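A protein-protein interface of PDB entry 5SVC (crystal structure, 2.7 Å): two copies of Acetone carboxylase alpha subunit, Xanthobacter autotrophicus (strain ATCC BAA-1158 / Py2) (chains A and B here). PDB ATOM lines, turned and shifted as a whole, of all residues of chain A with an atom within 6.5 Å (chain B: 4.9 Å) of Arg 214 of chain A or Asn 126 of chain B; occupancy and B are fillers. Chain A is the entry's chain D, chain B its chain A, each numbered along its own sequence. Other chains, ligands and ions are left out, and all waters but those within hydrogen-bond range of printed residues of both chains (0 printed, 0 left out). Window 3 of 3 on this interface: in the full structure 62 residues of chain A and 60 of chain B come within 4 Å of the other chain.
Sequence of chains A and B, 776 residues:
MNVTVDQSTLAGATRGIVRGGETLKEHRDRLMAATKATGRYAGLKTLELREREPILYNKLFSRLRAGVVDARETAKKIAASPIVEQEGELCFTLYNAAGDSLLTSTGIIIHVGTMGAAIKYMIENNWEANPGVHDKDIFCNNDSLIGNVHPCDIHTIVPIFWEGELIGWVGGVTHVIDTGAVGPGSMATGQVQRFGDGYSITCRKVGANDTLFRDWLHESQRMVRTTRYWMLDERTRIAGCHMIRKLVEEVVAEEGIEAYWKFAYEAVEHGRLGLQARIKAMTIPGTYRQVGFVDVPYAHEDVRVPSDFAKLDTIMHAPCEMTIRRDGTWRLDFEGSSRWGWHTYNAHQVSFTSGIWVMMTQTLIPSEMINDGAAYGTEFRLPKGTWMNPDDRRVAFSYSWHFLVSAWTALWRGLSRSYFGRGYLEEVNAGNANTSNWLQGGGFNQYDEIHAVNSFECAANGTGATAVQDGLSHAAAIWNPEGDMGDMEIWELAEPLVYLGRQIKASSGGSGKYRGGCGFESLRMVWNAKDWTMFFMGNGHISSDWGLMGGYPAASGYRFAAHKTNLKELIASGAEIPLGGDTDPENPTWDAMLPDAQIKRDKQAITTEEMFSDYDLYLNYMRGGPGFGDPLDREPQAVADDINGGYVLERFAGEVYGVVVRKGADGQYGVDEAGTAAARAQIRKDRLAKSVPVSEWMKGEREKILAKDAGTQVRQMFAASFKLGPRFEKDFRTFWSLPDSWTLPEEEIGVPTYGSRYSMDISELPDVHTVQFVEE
The backbone carbonyl oxygen (O) of Asn 125 of chain B lies close to the guanidinium group (NE) of Arg 214 of chain A (3.3 Å).
The side-chain amide nitrogen (ND2) of Asn 130 of chain B is in hydrogen-bond range of the backbone carbonyl oxygen (O) of Leu 212 of chain A (3.1 Å).
The side-chain amide oxygen (OD1) of Asn 130 of chain B sits at hydrogen-bond distance from the backbone NH (N) of Arg 214 of chain A, 2.9 Å away.
OD2 of Asp 767 of chain B lies within salt-bridge range of NE of Arg 214 of chain A (3.1 Å).
The side-chain carboxylate (OD2) of Asp 767 of chain B sits at hydrogen-bond distance from a ring nitrogen (NE2) of His 218 of chain A (3.1 Å).
The guanidinium group (NH1) of Arg 214 of chain A lies close to the backbone carbonyl oxygen (O) of Asn 126 of chain B, at 2.2 Å.
O of Met 122 of chain B sits at hydrogen-bond distance from N of Trp 127 of chain B.
The side-chain amide oxygen of Asn 125 of chain B lies close to the backbone carbonyl oxygen of Asp 767 of chain B (3.3 Å).
The backbone NH (N) of Ala 129 of chain B is in hydrogen-bond range of the side-chain amide oxygen (OD1) of Asn 126 of chain B (3.0 Å).
The backbone carbonyl oxygen (O) of Val 206 of chain A sits at hydrogen-bond distance from the backbone NH (N) of Phe 213 of chain A (2.9 Å).
Printed residues of chain A that touch a printed residue of chain B: Leu 212, Phe 213, Arg 214, Asp 215 and His 218.
Of the 11 printed residues of chain B, 6 touch a printed residue of chain A.
Hydrophobic or aromatic side chains of chain B within 4 Å of the printed part of chain A: Trp 127 and Pro 131.
Among the printed residues, Asp or Glu carboxylates within 4 Å of a Lys or Arg side-chain nitrogen of the other chain: Arg 214 of chain A with Asp 767 of chain B (3.1 Å).
Printed residues of chain B within 4 Å of Asp 215 of chain A: Trp 127 (3.6 Å) and Pro 131 (3.8 Å).
Printed residues of chain A within 4 Å of Asp 767 of chain B: Arg 214 and His 218.
Printed residues of chain A within 4 Å of Asn 125 of chain B: Arg 214 (3.1 Å) and His 218 (3.6 Å).
Printed residues of chain B within 4 Å of His 218 of chain A: Asn 125 (3.6 Å), Trp 127 (3.7 Å) and Asp 767 (3.1 Å).
Of the printed residues of chain A, Trp 127 of chain B touches Arg 214, Asp 215 and His 218.
Ile 123 of chain B touches none of the printed residues of chain A.
The nearest residue of chain B that does not touch Arg 214 of chain A is Ala 129 of chain B (4.03 Å).
The nearest printed residue of chain A that does not touch Asn 126 of chain B is His 218 of chain A (6.9 Å).
No position is printed for both chains.
Of the 12 pairs that touch across the chains among the printed residues, none has its exchanged pair printed and touching as well.
Among the printed residues, merely in contact across the chains: Phe 213 of chain A with Asn 130 of chain B, Arg 214 of chain A with Trp 127 of chain B, Asp 215 of chain A with Trp 127 of chain B, Asp 215 of chain A with Pro 131 of chain B, His 218 of chain A with Asn 125 of chain B and His 218 of chain A with Trp 127 of chain B.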
ATOM      1  N   VAL A 206     -27.116  16.432 -31.573  1.00  0.00           N
ATOM      2  CA  VAL A 206     -27.121  17.004 -30.246  1.00  0.00           C
ATOM      3  C   VAL A 206     -25.715  17.338 -29.794  1.00  0.00           C
ATOM      4  O   VAL A 206     -25.541  18.124 -28.843  1.00  0.00           O
ATOM      5  CB  VAL A 206     -27.812  16.015 -29.289  1.00  0.00           C
ATOM      6  CG1 VAL A 206     -27.110  15.895 -28.004  1.00  0.00           C
ATOM      7  CG2 VAL A 206     -29.295  16.387 -29.130  1.00  0.00           C
ATOM      8  N   LEU A 212     -21.629  18.252 -26.227  1.00  0.00           N
ATOM      9  CA  LEU A 212     -23.058  18.543 -26.357  1.00  0.00           C
ATOM     10  C   LEU A 212     -23.326  20.039 -26.587  1.00  0.00           C
ATOM     11  O   LEU A 212     -22.557  20.911 -26.190  1.00  0.00           O
ATOM     12  CB  LEU A 212     -23.802  18.077 -25.116  1.00  0.00           C
ATOM     13  CG  LEU A 212     -23.713  16.566 -24.887  1.00  0.00           C
ATOM     14  CD1 LEU A 212     -24.393  16.172 -23.604  1.00  0.00           C
ATOM     15  CD2 LEU A 212     -24.334  15.794 -26.044  1.00  0.00           C
ATOM     16  N   PHE A 213     -24.429  20.332 -27.252  1.00  0.00           N
ATOM     17  CA  PHE A 213     -24.799  21.699 -27.604  1.00  0.00           C
ATOM     18  C   PHE A 213     -25.587  22.344 -26.469  1.00  0.00           C
ATOM     19  O   PHE A 213     -26.579  21.770 -25.983  1.00  0.00           O
ATOM     20  CB  PHE A 213     -25.647  21.700 -28.867  1.00  0.00           C
ATOM     21  CG  PHE A 213     -24.901  21.298 -30.086  1.00  0.00           C
ATOM     22  CD1 PHE A 213     -23.663  21.820 -30.351  1.00  0.00           C
ATOM     23  CD2 PHE A 213     -25.430  20.365 -30.955  1.00  0.00           C
ATOM     24  CE1 PHE A 213     -22.961  21.443 -31.481  1.00  0.00           C
ATOM     25  CE2 PHE A 213     -24.736  19.969 -32.079  1.00  0.00           C
ATOM     26  CZ  PHE A 213     -23.499  20.517 -32.345  1.00  0.00           C
ATOM     27  N   ARG A 214     -25.189  23.569 -26.100  1.00  0.00           N
ATOM     28  CA  ARG A 214     -25.775  24.234 -24.939  1.00  0.00           C
ATOM     29  C   ARG A 214     -27.282  24.455 -25.100  1.00  0.00           C
ATOM     30  O   ARG A 214     -28.037  24.329 -24.125  1.00  0.00           O
ATOM     31  CB  ARG A 214     -25.045  25.555 -24.669  1.00  0.00           C
ATOM     32  CG  ARG A 214     -25.494  26.278 -23.378  1.00  0.00           C
ATOM     33  CD  ARG A 214     -24.666  27.551 -23.110  1.00  0.00           C
ATOM     34  NE  ARG A 214     -23.421  27.323 -22.354  1.00  0.00           N
ATOM     35  CZ  ARG A 214     -22.202  27.741 -22.715  1.00  0.00           C
ATOM     36  NH1 ARG A 214     -22.009  28.440 -23.834  1.00  0.00           N
ATOM     37  NH2 ARG A 214     -21.157  27.466 -21.938  1.00  0.00           N
ATOM     38  N   ASP A 215     -27.740  24.784 -26.320  1.00  0.00           N
ATOM     39  CA  ASP A 215     -29.175  24.999 -26.546  1.00  0.00           C
ATOM     40  C   ASP A 215     -29.974  23.708 -26.418  1.00  0.00           C
ATOM     41  O   ASP A 215     -31.155  23.744 -26.029  1.00  0.00           O
ATOM     42  CB  ASP A 215     -29.422  25.635 -27.920  1.00  0.00           C
ATOM     43  CG  ASP A 215     -28.750  24.863 -29.077  1.00  0.00           C
ATOM     44  OD1 ASP A 215     -27.683  24.255 -28.858  1.00  0.00           O
ATOM     45  OD2 ASP A 215     -29.285  24.882 -30.210  1.00  0.00           O
ATOM     46  N   TRP A 216     -29.339  22.563 -26.710  1.00  0.00           N
ATOM     47  CA  TRP A 216     -29.966  21.280 -26.415  1.00  0.00           C
ATOM     48  C   TRP A 216     -29.977  21.036 -24.927  1.00  0.00           C
ATOM     49  O   TRP A 216     -30.964  20.537 -24.391  1.00  0.00           O
ATOM     50  CB  TRP A 216     -29.247  20.148 -27.141  1.00  0.00           C
ATOM     51  CG  TRP A 216     -29.292  18.813 -26.491  1.00  0.00           C
ATOM     52  CD1 TRP A 216     -28.287  18.198 -25.795  1.00  0.00           C
ATOM     53  CD2 TRP A 216     -30.399  17.909 -26.454  1.00  0.00           C
ATOM     54  NE1 TRP A 216     -28.695  16.967 -25.340  1.00  0.00           N
ATOM     55  CE2 TRP A 216     -29.987  16.766 -25.743  1.00  0.00           C
ATOM     56  CE3 TRP A 216     -31.701  17.950 -26.955  1.00  0.00           C
ATOM     57  CZ2 TRP A 216     -30.832  15.695 -25.520  1.00  0.00           C
ATOM     58  CZ3 TRP A 216     -32.511  16.888 -26.739  1.00  0.00           C
ATOM     59  CH2 TRP A 216     -32.077  15.770 -26.032  1.00  0.00           C
ATOM     60  N   LEU A 217     -28.903  21.408 -24.241  1.00  0.00           N
ATOM     61  CA  LEU A 217     -28.807  21.162 -22.803  1.00  0.00           C
ATOM     62  C   LEU A 217     -29.889  21.912 -22.038  1.00  0.00           C
ATOM     63  O   LEU A 217     -30.581  21.337 -21.183  1.00  0.00           O
ATOM     64  CB  LEU A 217     -27.416  21.550 -22.306  1.00  0.00           C
ATOM     65  CG  LEU A 217     -26.393  20.613 -22.939  1.00  0.00           C
ATOM     66  CD1 LEU A 217     -25.029  21.266 -23.049  1.00  0.00           C
ATOM     67  CD2 LEU A 217     -26.336  19.263 -22.206  1.00  0.00           C
ATOM     68  N   HIS A 218     -30.013  23.215 -22.306  1.00  0.00           N
ATOM     69  CA  HIS A 218     -30.943  24.043 -21.555  1.00  0.00           C
ATOM     70  C   HIS A 218     -32.373  23.658 -21.855  1.00  0.00           C
ATOM     71  O   HIS A 218     -33.190  23.460 -20.944  1.00  0.00           O
ATOM     72  CB  HIS A 218     -30.710  25.514 -21.890  1.00  0.00           C
ATOM     73  CG  HIS A 218     -29.517  26.103 -21.208  1.00  0.00           C
ATOM     74  ND1 HIS A 218     -29.319  27.464 -21.101  1.00  0.00           N
ATOM     75  CD2 HIS A 218     -28.465  25.515 -20.589  1.00  0.00           C
ATOM     76  CE1 HIS A 218     -28.184  27.688 -20.460  1.00  0.00           C
ATOM     77  NE2 HIS A 218     -27.650  26.523 -20.131  1.00  0.00           N
ATOM     78  N   GLU A 219     -32.691  23.536 -23.137  1.00  0.00           N
ATOM     79  CA  GLU A 219     -34.047  23.192 -23.524  1.00  0.00           C
ATOM     80  C   GLU A 219     -34.438  21.840 -22.959  1.00  0.00           C
ATOM     81  O   GLU A 219     -35.436  21.723 -22.228  1.00  0.00           O
ATOM     82  CB  GLU A 219     -34.164  23.195 -25.036  1.00  0.00           C
ATOM     83  CG  GLU A 219     -35.394  22.508 -25.497  1.00  0.00           C
ATOM     84  CD  GLU A 219     -35.526  22.574 -26.968  1.00  0.00           C
ATOM     85  OE1 GLU A 219     -35.735  23.690 -27.472  1.00  0.00           O
ATOM     86  OE2 GLU A 219     -35.394  21.528 -27.616  1.00  0.00           O
ATOM     87  N   MET B 122     -29.345  34.476 -24.403  1.00  0.00           N
ATOM     88  CA  MET B 122     -28.198  33.926 -25.117  1.00  0.00           C
ATOM     89  C   MET B 122     -26.927  34.644 -24.674  1.00  0.00           C
ATOM     90  O   MET B 122     -25.935  34.009 -24.309  1.00  0.00           O
ATOM     91  CB  MET B 122     -28.402  34.022 -26.652  1.00  0.00           C
ATOM     92  CG  MET B 122     -29.539  33.148 -27.285  1.00  0.00           C
ATOM     93  SD  MET B 122     -29.617  32.933 -29.100  1.00  0.00           S
ATOM     94  CE  MET B 122     -30.408  34.445 -29.630  1.00  0.00           C
ATOM     95  N   ILE B 123     -26.974  35.980 -24.631  1.00  0.00           N
ATOM     96  CA  ILE B 123     -25.812  36.771 -24.222  1.00  0.00           C
ATOM     97  C   ILE B 123     -25.314  36.338 -22.849  1.00  0.00           C
ATOM     98  O   ILE B 123     -24.097  36.144 -22.644  1.00  0.00           O
ATOM     99  CB  ILE B 123     -26.164  38.270 -24.247  1.00  0.00           C
ATOM    100  CG1 ILE B 123     -26.495  38.704 -25.683  1.00  0.00           C
ATOM    101  CG2 ILE B 123     -25.059  39.094 -23.585  1.00  0.00           C
ATOM    102  CD1 ILE B 123     -26.614  40.208 -25.880  1.00  0.00           C
ATOM    103  N   GLU B 124     -26.255  36.131 -21.898  1.00  0.00           N
ATOM    104  CA  GLU B 124     -25.942  35.881 -20.497  1.00  0.00           C
ATOM    105  C   GLU B 124     -25.563  34.443 -20.226  1.00  0.00           C
ATOM    106  O   GLU B 124     -25.010  34.159 -19.158  1.00  0.00           O
ATOM    107  CB  GLU B 124     -27.119  36.250 -19.577  1.00  0.00           C
ATOM    108  CG  GLU B 124     -27.211  37.720 -19.244  1.00  0.00           C
ATOM    109  CD  GLU B 124     -26.036  38.180 -18.387  1.00  0.00           C
ATOM    110  OE1 GLU B 124     -25.752  37.519 -17.359  1.00  0.00           O
ATOM    111  OE2 GLU B 124     -25.386  39.188 -18.762  1.00  0.00           O
ATOM    112  N   ASN B 125     -25.869  33.529 -21.135  1.00  0.00           N
ATOM    113  CA  ASN B 125     -25.536  32.130 -20.946  1.00  0.00           C
ATOM    114  C   ASN B 125     -24.476  31.683 -21.916  1.00  0.00           C
ATOM    115  O   ASN B 125     -24.320  30.482 -22.131  1.00  0.00           O
ATOM    116  CB  ASN B 125     -26.778  31.266 -21.078  1.00  0.00           C
ATOM    117  CG  ASN B 125     -27.804  31.615 -20.048  1.00  0.00           C
ATOM    118  OD1 ASN B 125     -27.850  31.002 -18.974  1.00  0.00           O
ATOM    119  ND2 ASN B 125     -28.606  32.647 -20.335  1.00  0.00           N
ATOM    120  N   ASN B 126     -23.763  32.635 -22.520  1.00  0.00           N
ATOM    121  CA  ASN B 126     -22.543  32.343 -23.263  1.00  0.00           C
ATOM    122  C   ASN B 126     -22.839  31.424 -24.445  1.00  0.00           C
ATOM    123  O   ASN B 126     -22.081  30.495 -24.732  1.00  0.00           O
ATOM    124  CB  ASN B 126     -21.459  31.755 -22.347  1.00  0.00           C
ATOM    125  CG  ASN B 126     -20.062  31.746 -22.996  1.00  0.00           C
ATOM    126  OD1 ASN B 126     -19.828  32.408 -24.002  1.00  0.00           O
ATOM    127  ND2 ASN B 126     -19.136  30.970 -22.413  1.00  0.00           N
ATOM    128  N   TRP B 127     -23.980  31.664 -25.110  1.00  0.00           N
ATOM    129  CA  TRP B 127     -24.213  31.062 -26.421  1.00  0.00           C
ATOM    130  C   TRP B 127     -23.018  31.320 -27.319  1.00  0.00           C
ATOM    131  O   TRP B 127     -22.737  30.538 -28.233  1.00  0.00           O
ATOM    132  CB  TRP B 127     -25.448  31.666 -27.080  1.00  0.00           C
ATOM    133  CG  TRP B 127     -26.688  30.839 -27.238  1.00  0.00           C
ATOM    134  CD1 TRP B 127     -27.425  30.677 -28.383  1.00  0.00           C
ATOM    135  CD2 TRP B 127     -27.385  30.126 -26.215  1.00  0.00           C
ATOM    136  NE1 TRP B 127     -28.532  29.902 -28.134  1.00  0.00           N
ATOM    137  CE2 TRP B 127     -28.522  29.540 -26.814  1.00  0.00           C
ATOM    138  CE3 TRP B 127     -27.143  29.901 -24.858  1.00  0.00           C
ATOM    139  CZ2 TRP B 127     -29.412  28.758 -26.096  1.00  0.00           C
ATOM    140  CZ3 TRP B 127     -28.007  29.135 -24.163  1.00  0.00           C
ATOM    141  CH2 TRP B 127     -29.143  28.573 -24.770  1.00  0.00           C
ATOM    142  N   GLU B 128     -22.301  32.416 -27.057  1.00  0.00           N
ATOM    143  CA  GLU B 128     -21.153  32.767 -27.872  1.00  0.00           C
ATOM    144  C   GLU B 128     -20.134  31.636 -27.900  1.00  0.00           C
ATOM    145  O   GLU B 128     -19.656  31.240 -28.970  1.00  0.00           O
ATOM    146  CB  GLU B 128     -20.535  34.062 -27.349  1.00  0.00           C
ATOM    147  CG  GLU B 128     -19.381  34.535 -28.181  1.00  0.00           C
ATOM    148  CD  GLU B 128     -18.966  35.931 -27.860  1.00  0.00           C
ATOM    149  OE1 GLU B 128     -19.668  36.600 -27.067  1.00  0.00           O
ATOM    150  OE2 GLU B 128     -17.949  36.369 -28.438  1.00  0.00           O
ATOM    151  N   ALA B 129     -19.792  31.095 -26.734  1.00  0.00           N
ATOM    152  CA  ALA B 129     -18.889  29.948 -26.708  1.00  0.00           C
ATOM    153  C   ALA B 129     -19.530  28.707 -27.324  1.00  0.00           C
ATOM    154  O   ALA B 129     -18.853  27.929 -28.002  1.00  0.00           O
ATOM    155  CB  ALA B 129     -18.453  29.661 -25.279  1.00  0.00           C
ATOM    156  N   ASN B 130     -20.827  28.497 -27.082  1.00  0.00           N
ATOM    157  CA  ASN B 130     -21.535  27.283 -27.460  1.00  0.00           C
ATOM    158  C   ASN B 130     -23.013  27.566 -27.412  1.00  0.00           C
ATOM    159  O   ASN B 130     -23.508  27.849 -26.332  1.00  0.00           O
ATOM    160  CB  ASN B 130     -21.176  26.174 -26.476  1.00  0.00           C
ATOM    161  CG  ASN B 130     -21.899  24.870 -26.740  1.00  0.00           C
ATOM    162  OD1 ASN B 130     -22.932  24.826 -27.393  1.00  0.00           O
ATOM    163  ND2 ASN B 130     -21.348  23.781 -26.195  1.00  0.00           N
ATOM    164  N   PRO B 131     -23.749  27.399 -28.535  1.00  0.00           N
ATOM    165  CA  PRO B 131     -23.376  26.759 -29.796  1.00  0.00           C
ATOM    166  C   PRO B 131     -22.689  27.703 -30.798  1.00  0.00           C
ATOM    167  O   PRO B 131     -22.410  27.317 -31.932  1.00  0.00           O
ATOM    168  CB  PRO B 131     -24.725  26.261 -30.317  1.00  0.00           C
ATOM    169  CG  PRO B 131     -25.632  27.296 -29.906  1.00  0.00           C
ATOM    170  CD  PRO B 131     -25.147  27.855 -28.593  1.00  0.00           C
ATOM    171  N   ASP B 767     -26.415  25.508 -15.180  1.00  0.00           N
ATOM    172  CA  ASP B 767     -25.930  26.457 -16.185  1.00  0.00           C
ATOM    173  C   ASP B 767     -26.936  27.544 -16.533  1.00  0.00           C
ATOM    174  O   ASP B 767     -26.711  28.310 -17.478  1.00  0.00           O
ATOM    175  CB  ASP B 767     -25.461  25.765 -17.471  1.00  0.00           C
ATOM    176  CG  ASP B 767     -24.563  26.668 -18.334  1.00  0.00           C
ATOM    177  OD1 ASP B 767     -23.785  27.458 -17.764  1.00  0.00           O
ATOM    178  OD2 ASP B 767     -24.625  26.596 -19.578  1.00  0.00           O
